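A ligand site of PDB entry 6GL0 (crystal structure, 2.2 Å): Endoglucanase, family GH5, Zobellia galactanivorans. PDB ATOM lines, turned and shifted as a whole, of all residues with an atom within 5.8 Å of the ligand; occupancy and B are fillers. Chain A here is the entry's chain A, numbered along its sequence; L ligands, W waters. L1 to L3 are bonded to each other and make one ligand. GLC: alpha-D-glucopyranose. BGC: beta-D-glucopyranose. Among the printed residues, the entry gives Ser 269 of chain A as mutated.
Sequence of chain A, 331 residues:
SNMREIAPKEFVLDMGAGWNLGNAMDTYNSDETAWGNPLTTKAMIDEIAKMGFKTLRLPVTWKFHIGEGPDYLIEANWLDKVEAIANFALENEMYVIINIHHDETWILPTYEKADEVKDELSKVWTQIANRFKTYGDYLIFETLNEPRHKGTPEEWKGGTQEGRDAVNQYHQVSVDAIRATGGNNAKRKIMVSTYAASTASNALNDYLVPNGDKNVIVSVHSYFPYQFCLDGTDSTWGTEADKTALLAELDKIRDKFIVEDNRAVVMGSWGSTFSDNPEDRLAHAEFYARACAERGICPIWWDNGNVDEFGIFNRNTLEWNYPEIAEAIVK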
ATOM      1  N   ASN A  23      12.176 -12.180  10.502  1.00  0.00           N
ATOM      2  CA  ASN A  23      12.279 -13.292   9.569  1.00  0.00           C
ATOM      3  C   ASN A  23      13.255 -14.372  10.021  1.00  0.00           C
ATOM      4  O   ASN A  23      14.044 -14.848   9.238  1.00  0.00           O
ATOM      5  CB  ASN A  23      12.566 -12.777   8.152  1.00  0.00           C
ATOM      6  CG  ASN A  23      11.345 -12.196   7.468  1.00  0.00           C
ATOM      7  OD1 ASN A  23      10.295 -11.965   8.088  1.00  0.00           O
ATOM      8  ND2 ASN A  23      11.496 -11.906   6.177  1.00  0.00           N
ATOM      9  N   ASP A  26      10.252 -16.145  13.708  1.00  0.00           N
ATOM     10  CA  ASP A  26       8.909 -15.759  13.248  1.00  0.00           C
ATOM     11  C   ASP A  26       8.551 -16.296  11.860  1.00  0.00           C
ATOM     12  O   ASP A  26       7.407 -16.218  11.459  1.00  0.00           O
ATOM     13  CB  ASP A  26       8.731 -14.230  13.315  1.00  0.00           C
ATOM     14  CG  ASP A  26       9.855 -13.469  12.651  1.00  0.00           C
ATOM     15  OD1 ASP A  26      11.039 -13.743  12.970  1.00  0.00           O
ATOM     16  OD2 ASP A  26       9.576 -12.644  11.762  1.00  0.00           O
ATOM     17  N   ALA A  34      13.841 -20.686   6.169  1.00  0.00           N
ATOM     18  CA  ALA A  34      13.147 -20.658   4.880  1.00  0.00           C
ATOM     19  C   ALA A  34      12.878 -19.267   4.326  1.00  0.00           C
ATOM     20  O   ALA A  34      12.616 -19.119   3.129  1.00  0.00           O
ATOM     21  CB  ALA A  34      11.835 -21.416   4.972  1.00  0.00           C
ATOM     22  N   TRP A  35      12.967 -18.234   5.169  1.00  0.00           N
ATOM     23  CA  TRP A  35      12.740 -16.845   4.713  1.00  0.00           C
ATOM     24  C   TRP A  35      14.048 -16.067   4.553  1.00  0.00           C
ATOM     25  O   TRP A  35      14.057 -14.838   4.569  1.00  0.00           O
ATOM     26  CB  TRP A  35      11.755 -16.150   5.638  1.00  0.00           C
ATOM     27  CG  TRP A  35      10.319 -16.488   5.368  1.00  0.00           C
ATOM     28  CD1 TRP A  35       9.825 -17.431   4.500  1.00  0.00           C
ATOM     29  CD2 TRP A  35       9.196 -15.902   6.015  1.00  0.00           C
ATOM     30  NE1 TRP A  35       8.445 -17.451   4.555  1.00  0.00           N
ATOM     31  CE2 TRP A  35       8.036 -16.531   5.478  1.00  0.00           C
ATOM     32  CE3 TRP A  35       9.048 -14.905   6.989  1.00  0.00           C
ATOM     33  CZ2 TRP A  35       6.722 -16.153   5.870  1.00  0.00           C
ATOM     34  CZ3 TRP A  35       7.746 -14.548   7.414  1.00  0.00           C
ATOM     35  CH2 TRP A  35       6.597 -15.167   6.834  1.00  0.00           C
ATOM     36  N   GLY A  36      15.138 -16.810   4.335  1.00  0.00           N
ATOM     37  CA  GLY A  36      16.389 -16.241   3.863  1.00  0.00           C
ATOM     38  C   GLY A  36      17.377 -15.841   4.955  1.00  0.00           C
ATOM     39  O   GLY A  36      18.434 -15.298   4.646  1.00  0.00           O
ATOM     40  N   ARG A  57      14.253  -7.588  20.272  1.00  0.00           N
ATOM     41  CA  ARG A  57      12.955  -8.229  20.090  1.00  0.00           C
ATOM     42  C   ARG A  57      13.221  -9.497  19.296  1.00  0.00           C
ATOM     43  O   ARG A  57      13.852  -9.461  18.228  1.00  0.00           O
ATOM     44  CB  ARG A  57      11.966  -7.336  19.348  1.00  0.00           C
ATOM     45  CG  ARG A  57      10.581  -7.894  19.302  1.00  0.00           C
ATOM     46  CD  ARG A  57       9.572  -6.769  19.272  1.00  0.00           C
ATOM     47  NE  ARG A  57       8.178  -7.161  19.021  1.00  0.00           N
ATOM     48  CZ  ARG A  57       7.645  -7.353  17.802  1.00  0.00           C
ATOM     49  NH1 ARG A  57       8.373  -7.272  16.715  1.00  0.00           N
ATOM     50  NH2 ARG A  57       6.351  -7.641  17.690  1.00  0.00           N
ATOM     51  N   HIS A 101       3.931 -14.490  17.330  1.00  0.00           N
ATOM     52  CA  HIS A 101       4.056 -13.691  16.098  1.00  0.00           C
ATOM     53  C   HIS A 101       3.040 -14.128  15.023  1.00  0.00           C
ATOM     54  O   HIS A 101       1.868 -13.773  15.168  1.00  0.00           O
ATOM     55  CB  HIS A 101       5.494 -13.624  15.582  1.00  0.00           C
ATOM     56  CG  HIS A 101       5.799 -12.388  14.815  1.00  0.00           C
ATOM     57  ND1 HIS A 101       6.142 -11.197  15.430  1.00  0.00           N
ATOM     58  CD2 HIS A 101       5.836 -12.142  13.482  1.00  0.00           C
ATOM     59  CE1 HIS A 101       6.367 -10.271  14.506  1.00  0.00           C
ATOM     60  NE2 HIS A 101       6.213 -10.830  13.322  1.00  0.00           N
ATOM     61  N   HIS A 102       3.434 -14.860  13.957  1.00  0.00           N
ATOM     62  CA  HIS A 102       2.525 -15.092  12.806  1.00  0.00           C
ATOM     63  C   HIS A 102       1.648 -16.324  13.061  1.00  0.00           C
ATOM     64  O   HIS A 102       1.663 -17.270  12.267  1.00  0.00           O
ATOM     65  CB  HIS A 102       3.285 -15.325  11.496  1.00  0.00           C
ATOM     66  CG  HIS A 102       4.029 -14.157  10.985  1.00  0.00           C
ATOM     67  ND1 HIS A 102       3.440 -12.902  10.849  1.00  0.00           N
ATOM     68  CD2 HIS A 102       5.292 -14.049  10.502  1.00  0.00           C
ATOM     69  CE1 HIS A 102       4.326 -12.080  10.324  1.00  0.00           C
ATOM     70  NE2 HIS A 102       5.457 -12.755  10.085  1.00  0.00           N
ATOM     71  N   ASN A 145       1.425 -10.385  18.729  1.00  0.00           N
ATOM     72  CA  ASN A 145       2.131  -9.470  17.863  1.00  0.00           C
ATOM     73  C   ASN A 145       1.214  -8.402  17.290  1.00  0.00           C
ATOM     74  O   ASN A 145       1.329  -7.241  17.642  1.00  0.00           O
ATOM     75  CB  ASN A 145       2.892 -10.216  16.728  1.00  0.00           C
ATOM     76  CG  ASN A 145       3.503  -9.278  15.691  1.00  0.00           C
ATOM     77  OD1 ASN A 145       4.164  -8.314  16.049  1.00  0.00           O
ATOM     78  ND2 ASN A 145       3.308  -9.571  14.414  1.00  0.00           N
ATOM     79  N   GLU A 146       0.395  -8.836  16.335  1.00  0.00           N
ATOM     80  CA  GLU A 146      -0.559  -8.000  15.620  1.00  0.00           C
ATOM     81  C   GLU A 146      -1.890  -8.748  15.478  1.00  0.00           C
ATOM     82  O   GLU A 146      -2.303  -9.069  14.370  1.00  0.00           O
ATOM     83  CB  GLU A 146       0.047  -7.584  14.271  1.00  0.00           C
ATOM     84  CG  GLU A 146       1.281  -6.705  14.413  1.00  0.00           C
ATOM     85  CD  GLU A 146       1.792  -6.123  13.109  1.00  0.00           C
ATOM     86  OE1 GLU A 146       1.459  -6.666  12.019  1.00  0.00           O
ATOM     87  OE2 GLU A 146       2.526  -5.109  13.150  1.00  0.00           O
ATOM     88  N   HIS A 221       2.671  -0.648  16.895  1.00  0.00           N
ATOM     89  CA  HIS A 221       3.583  -0.595  15.760  1.00  0.00           C
ATOM     90  C   HIS A 221       3.074   0.508  14.828  1.00  0.00           C
ATOM     91  O   HIS A 221       1.889   0.635  14.609  1.00  0.00           O
ATOM     92  CB  HIS A 221       3.582  -1.929  14.985  1.00  0.00           C
ATOM     93  CG  HIS A 221       3.966  -3.109  15.807  1.00  0.00           C
ATOM     94  ND1 HIS A 221       3.718  -4.402  15.389  1.00  0.00           N
ATOM     95  CD2 HIS A 221       4.547  -3.222  17.025  1.00  0.00           C
ATOM     96  CE1 HIS A 221       4.131  -5.256  16.310  1.00  0.00           C
ATOM     97  NE2 HIS A 221       4.625  -4.570  17.323  1.00  0.00           N
ATOM     98  N   TYR A 223       4.371   2.154  11.316  1.00  0.00           N
ATOM     99  CA  TYR A 223       5.296   2.349  10.190  1.00  0.00           C
ATOM    100  C   TYR A 223       4.943   3.677   9.471  1.00  0.00           C
ATOM    101  O   TYR A 223       4.495   3.681   8.311  1.00  0.00           O
ATOM    102  CB  TYR A 223       5.198   1.132   9.237  1.00  0.00           C
ATOM    103  CG  TYR A 223       5.756  -0.149   9.797  1.00  0.00           C
ATOM    104  CD1 TYR A 223       4.989  -0.978  10.565  1.00  0.00           C
ATOM    105  CD2 TYR A 223       7.096  -0.517   9.550  1.00  0.00           C
ATOM    106  CE1 TYR A 223       5.499  -2.180  11.023  1.00  0.00           C
ATOM    107  CE2 TYR A 223       7.630  -1.691  10.013  1.00  0.00           C
ATOM    108  CZ  TYR A 223       6.842  -2.526  10.758  1.00  0.00           C
ATOM    109  OH  TYR A 223       7.364  -3.706  11.221  1.00  0.00           O
ATOM    110  N   LEU A 230       6.147   1.173   4.114  1.00  0.00           N
ATOM    111  CA  LEU A 230       5.703  -0.127   3.734  1.00  0.00           C
ATOM    112  C   LEU A 230       5.437  -0.302   2.259  1.00  0.00           C
ATOM    113  O   LEU A 230       5.871  -1.296   1.709  1.00  0.00           O
ATOM    114  CB  LEU A 230       4.440  -0.481   4.525  1.00  0.00           C
ATOM    115  CG  LEU A 230       4.611  -0.756   6.019  1.00  0.00           C
ATOM    116  CD1 LEU A 230       3.227  -0.793   6.688  1.00  0.00           C
ATOM    117  CD2 LEU A 230       5.405  -2.048   6.225  1.00  0.00           C
ATOM    118  N   SER A 269       7.749  -2.229  16.619  1.00  0.00           N
ATOM    119  CA  SER A 269       8.107  -2.324  15.218  1.00  0.00           C
ATOM    120  C   SER A 269       7.784  -1.044  14.524  1.00  0.00           C
ATOM    121  O   SER A 269       6.715  -0.467  14.740  1.00  0.00           O
ATOM    122  CB  SER A 269       7.325  -3.436  14.511  1.00  0.00           C
ATOM    123  OG  SER A 269       7.951  -4.645  14.701  1.00  0.00           O
ATOM    124  N   TRP A 302      12.412  -2.650  12.783  1.00  0.00           N
ATOM    125  CA  TRP A 302      12.095  -3.921  12.161  1.00  0.00           C
ATOM    126  C   TRP A 302      13.152  -4.236  11.123  1.00  0.00           C
ATOM    127  O   TRP A 302      13.384  -3.454  10.177  1.00  0.00           O
ATOM    128  CB  TRP A 302      10.711  -3.882  11.482  1.00  0.00           C
ATOM    129  CG  TRP A 302      10.427  -5.164  10.771  1.00  0.00           C
ATOM    130  CD1 TRP A 302      10.423  -5.374   9.437  1.00  0.00           C
ATOM    131  CD2 TRP A 302      10.190  -6.414  11.382  1.00  0.00           C
ATOM    132  NE1 TRP A 302      10.196  -6.704   9.184  1.00  0.00           N
ATOM    133  CE2 TRP A 302      10.043  -7.363  10.371  1.00  0.00           C
ATOM    134  CE3 TRP A 302      10.117  -6.829  12.699  1.00  0.00           C
ATOM    135  CZ2 TRP A 302       9.787  -8.709  10.634  1.00  0.00           C
ATOM    136  CZ3 TRP A 302       9.908  -8.170  12.967  1.00  0.00           C
ATOM    137  CH2 TRP A 302       9.723  -9.084  11.947  1.00  0.00           C
ATOM    138  N   ASN A 304      14.349  -7.411   8.685  1.00  0.00           N
ATOM    139  CA  ASN A 304      13.981  -8.750   8.175  1.00  0.00           C
ATOM    140  C   ASN A 304      15.137  -9.483   7.531  1.00  0.00           C
ATOM    141  O   ASN A 304      14.961 -10.514   6.895  1.00  0.00           O
ATOM    142  CB  ASN A 304      12.754  -8.676   7.256  1.00  0.00           C
ATOM    143  CG  ASN A 304      13.063  -8.051   5.903  1.00  0.00           C
ATOM    144  OD1 ASN A 304      14.127  -7.387   5.692  1.00  0.00           O
ATOM    145  ND2 ASN A 304      12.143  -8.308   4.949  1.00  0.00           N
ATOM    146  N   ASN A 306      16.912  -8.729   4.960  1.00  0.00           N
ATOM    147  CA  ASN A 306      17.069  -8.566   3.508  1.00  0.00           C
ATOM    148  C   ASN A 306      17.382  -7.112   3.242  1.00  0.00           C
ATOM    149  O   ASN A 306      16.548  -6.231   3.473  1.00  0.00           O
ATOM    150  CB  ASN A 306      15.771  -8.944   2.806  1.00  0.00           C
ATOM    151  CG  ASN A 306      15.825  -8.762   1.291  1.00  0.00           C
ATOM    152  OD1 ASN A 306      16.650  -8.083   0.723  1.00  0.00           O
ATOM    153  ND2 ASN A 306      14.899  -9.417   0.624  1.00  0.00           N
ATOM    154  N   GLU A 309      15.086  -4.639   1.590  1.00  0.00           N
ATOM    155  CA  GLU A 309      13.807  -4.365   2.295  1.00  0.00           C
ATOM    156  C   GLU A 309      14.141  -3.667   3.606  1.00  0.00           C
ATOM    157  O   GLU A 309      14.431  -2.488   3.586  1.00  0.00           O
ATOM    158  CB  GLU A 309      12.985  -5.642   2.455  1.00  0.00           C
ATOM    159  CG  GLU A 309      12.455  -6.157   1.111  1.00  0.00           C
ATOM    160  CD  GLU A 309      11.814  -7.550   1.155  1.00  0.00           C
ATOM    161  OE1 GLU A 309      11.711  -8.207   2.203  1.00  0.00           O
ATOM    162  OE2 GLU A 309      11.433  -8.002   0.069  1.00  0.00           O
ATOM    163  N   PHE A 310      14.149  -4.382   4.739  1.00  0.00           N
ATOM    164  CA  PHE A 310      14.326  -3.795   6.043  1.00  0.00           C
ATOM    165  C   PHE A 310      15.688  -4.107   6.680  1.00  0.00           C
ATOM    166  O   PHE A 310      15.999  -3.623   7.784  1.00  0.00           O
ATOM    167  CB  PHE A 310      13.186  -4.255   6.999  1.00  0.00           C
ATOM    168  CG  PHE A 310      11.851  -3.631   6.685  1.00  0.00           C
ATOM    169  CD1 PHE A 310      11.551  -2.355   7.157  1.00  0.00           C
ATOM    170  CD2 PHE A 310      10.900  -4.298   5.916  1.00  0.00           C
ATOM    171  CE1 PHE A 310      10.310  -1.777   6.917  1.00  0.00           C
ATOM    172  CE2 PHE A 310       9.659  -3.717   5.633  1.00  0.00           C
ATOM    173  CZ  PHE A 310       9.366  -2.428   6.147  1.00  0.00           C
HETATM  174  C1  GLC L   1       4.906  -6.138  11.117  1.00  0.00           C
HETATM  175  C2  GLC L   1       4.976  -7.669  11.190  1.00  0.00           C
HETATM  176  C3  GLC L   1       6.227  -8.235  10.546  1.00  0.00           C
HETATM  177  C4  GLC L   1       6.352  -7.674   9.148  1.00  0.00           C
HETATM  178  C5  GLC L   1       6.434  -6.163   9.273  1.00  0.00           C
HETATM  179  C6  GLC L   1       6.589  -5.424   7.945  1.00  0.00           C
HETATM  180  O1  GLC L   1       5.781  -5.473  12.043  1.00  0.00           O
HETATM  181  O2  GLC L   1       4.916  -8.013  12.577  1.00  0.00           O
HETATM  182  O3  GLC L   1       6.139  -9.645  10.527  1.00  0.00           O
HETATM  183  O4  GLC L   1       7.528  -8.160   8.535  1.00  0.00           O
HETATM  184  O5  GLC L   1       5.203  -5.735   9.824  1.00  0.00           O
HETATM  185  O6  GLC L   1       5.489  -5.744   7.111  1.00  0.00           O
HETATM  186  C2  BGC L   2       8.651  -9.006   6.654  1.00  0.00           C
HETATM  187  C3  BGC L   2       8.453  -9.653   5.292  1.00  0.00           C
HETATM  188  C4  BGC L   2       7.583 -10.892   5.377  1.00  0.00           C
HETATM  189  C5  BGC L   2       6.315 -10.529   6.128  1.00  0.00           C
HETATM  190  C6  BGC L   2       5.465 -11.750   6.413  1.00  0.00           C
HETATM  191  C1  BGC L   2       7.294  -8.697   7.239  1.00  0.00           C
HETATM  192  O2  BGC L   2       9.398  -7.821   6.500  1.00  0.00           O
HETATM  193  O3  BGC L   2       9.716  -9.918   4.734  1.00  0.00           O
HETATM  194  O4  BGC L   2       7.206 -11.306   4.062  1.00  0.00           O
HETATM  195  O5  BGC L   2       6.558  -9.872   7.349  1.00  0.00           O
HETATM  196  O6  BGC L   2       4.126 -11.345   6.662  1.00  0.00           O
HETATM  197  C2  BGC L   3       6.655 -13.164   2.590  1.00  0.00           C
HETATM  198  C3  BGC L   3       7.115 -14.521   2.052  1.00  0.00           C
HETATM  199  C4  BGC L   3       8.611 -14.428   1.718  1.00  0.00           C
HETATM  200  C5  BGC L   3       9.386 -13.942   2.940  1.00  0.00           C
HETATM  201  C6  BGC L   3      10.879 -13.741   2.733  1.00  0.00           C
HETATM  202  C1  BGC L   3       7.552 -12.658   3.721  1.00  0.00           C
HETATM  203  O2  BGC L   3       5.351 -13.326   3.054  1.00  0.00           O
HETATM  204  O3  BGC L   3       6.327 -14.934   0.933  1.00  0.00           O
HETATM  205  O4  BGC L   3       9.121 -15.695   1.351  1.00  0.00           O
HETATM  206  O5  BGC L   3       8.899 -12.701   3.348  1.00  0.00           O
HETATM  207  O6  BGC L   3      11.142 -12.755   1.754  1.00  0.00           O
HETATM  208  O   HOH W   1       2.866  -6.374   7.875  1.00  0.00           O
HETATM  209  O   HOH W   2      13.387 -11.168   2.448  1.00  0.00           O
HETATM  210  O   HOH W   3      10.149 -10.082   2.045  1.00  0.00           O
HETATM  211  O   HOH W   4       5.600  -5.203   4.400  1.00  0.00           O
HETATM  212  O   HOH W   5       6.739  -6.766  14.046  1.00  0.00           O
HETATM  213  O   HOH W   6       7.990 -11.653   9.782  1.00  0.00           O
HETATM  214  O   HOH W   7       4.060 -15.263   0.030  1.00  0.00           O
HETATM  215  O   HOH W   8       9.280  -6.824   3.965  1.00  0.00           O
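O1 of GLC L1 lies within hydrogen-bond range of OH of Tyr 223, 2.5 Å away. O2 of GLC L1 sits at hydrogen-bond distance from ND2 of Asn 145 (2.9 Å). An oxygen (O3) of BGC L2 lies within hydrogen-bond range of the side-chain amide nitrogen (ND2) of Asn 304 (2.9 Å). NE1 of Trp 302 is in hydrogen-bond range of O2 of BGC L2 (3.0 Å). The side-chain amide nitrogen (ND2) of Asn 23 is in hydrogen-bond range of an oxygen (O3) of BGC L2 (3.0 Å). O3 of GLC L1 is in hydrogen-bond range of NE2 of His 101 (3.0 Å). An oxygen (O3) of GLC L1 lies close to a ring nitrogen (NE2) of His 102. The side-chain carboxylate of Glu 146 sits close to an oxygen (O1) of GLC L1 (3.5 Å).
ND2 of Asn 145 sits close to NE2 of His 101, 3.3 Å away. The side-chain amide oxygen (OD1) of Asn 145 is in hydrogen-bond range of the guanidinium group (NH2) of Arg 57, at 2.8 Å. The side-chain carboxylate of Glu 309 is in hydrogen-bond range of the side-chain amide nitrogen of Asn 304. The backbone NH (N) of Phe 310 lies within hydrogen-bond range of the side-chain amide oxygen (OD1) of Asn 304, at 3.2 Å. N of Asn 306 is in hydrogen-bond range of OD1 of Asn 304 (3.2 Å). The side-chain carboxylate (OD2) of Asp 26 is in hydrogen-bond range of the backbone NH (N) of Asn 23, at 2.9 Å. A ring nitrogen (ND1) of His 221 is in hydrogen-bond range of the side-chain carboxylate (OE2) of Glu 146 (2.6 Å). NH1 of Arg 57 sits at hydrogen-bond distance from OG of Ser 269.
CH2 of Trp 35 touches C6 of BGC L2, 3.6 Å away. CD2 of Leu 230 touches O6 of GLC L1, at 3.8 Å. OG of Ser 269 touches O1 of GLC L1 (3.5 Å). OE1 of Glu 309 touches O3 of BGC L2, 3.6 Å away. CD2 of Phe 310 touches O2 of BGC L2, 3.9 Å away. Hydrophobic or aromatic side chains within 4 Å of the ligand: Trp 35, His 101, His 102, Tyr 223, Leu 230, Trp 302 and Phe 310. Within 4 Å of the ligand: Asn 23, Trp 35, His 101, His 102, Asn 145, Glu 146, Tyr 223, Leu 230, Ser 269, Trp 302, Asn 304, Glu 309 and Phe 310. Along chain A the residues within 4 Å of the ligand span positions 23 to 310. The nearest printed residue that does not touch the ligand is His 221 (4.1 Å).
Water W5 lies within hydrogen-bond range of OG of Ser 269 (2.5 Å), O1 of GLC L1 (2.6 Å) and NH1 of Arg 57 (3.2 Å). Water W8 lies within hydrogen-bond range of an oxygen (O2) of BGC L2 (2.7 Å), the side-chain carboxylate (OE1) of Glu 309 (3.3 Å) and the side-chain amide nitrogen (ND2) of Asn 304 (3.4 Å). Water W3 bridges OE1 of Glu 309 (2.4 Å) and O3 of BGC L2 (2.7 Å). Water W6 lies within hydrogen-bond range of OD2 of Asp 26 (2.7 Å), NE2 of His 102 (2.8 Å), O3 of GLC L1 (2.8 Å) and OD1 of Asn 23 (2.9 Å). Water W2 lies within hydrogen-bond range of an oxygen (O6) of BGC L3 (2.8 Å), the side-chain amide nitrogen (ND2) of Asn 306 (2.9 Å) and the side-chain carboxylate (OE1) of Glu 309 (3.4 Å).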
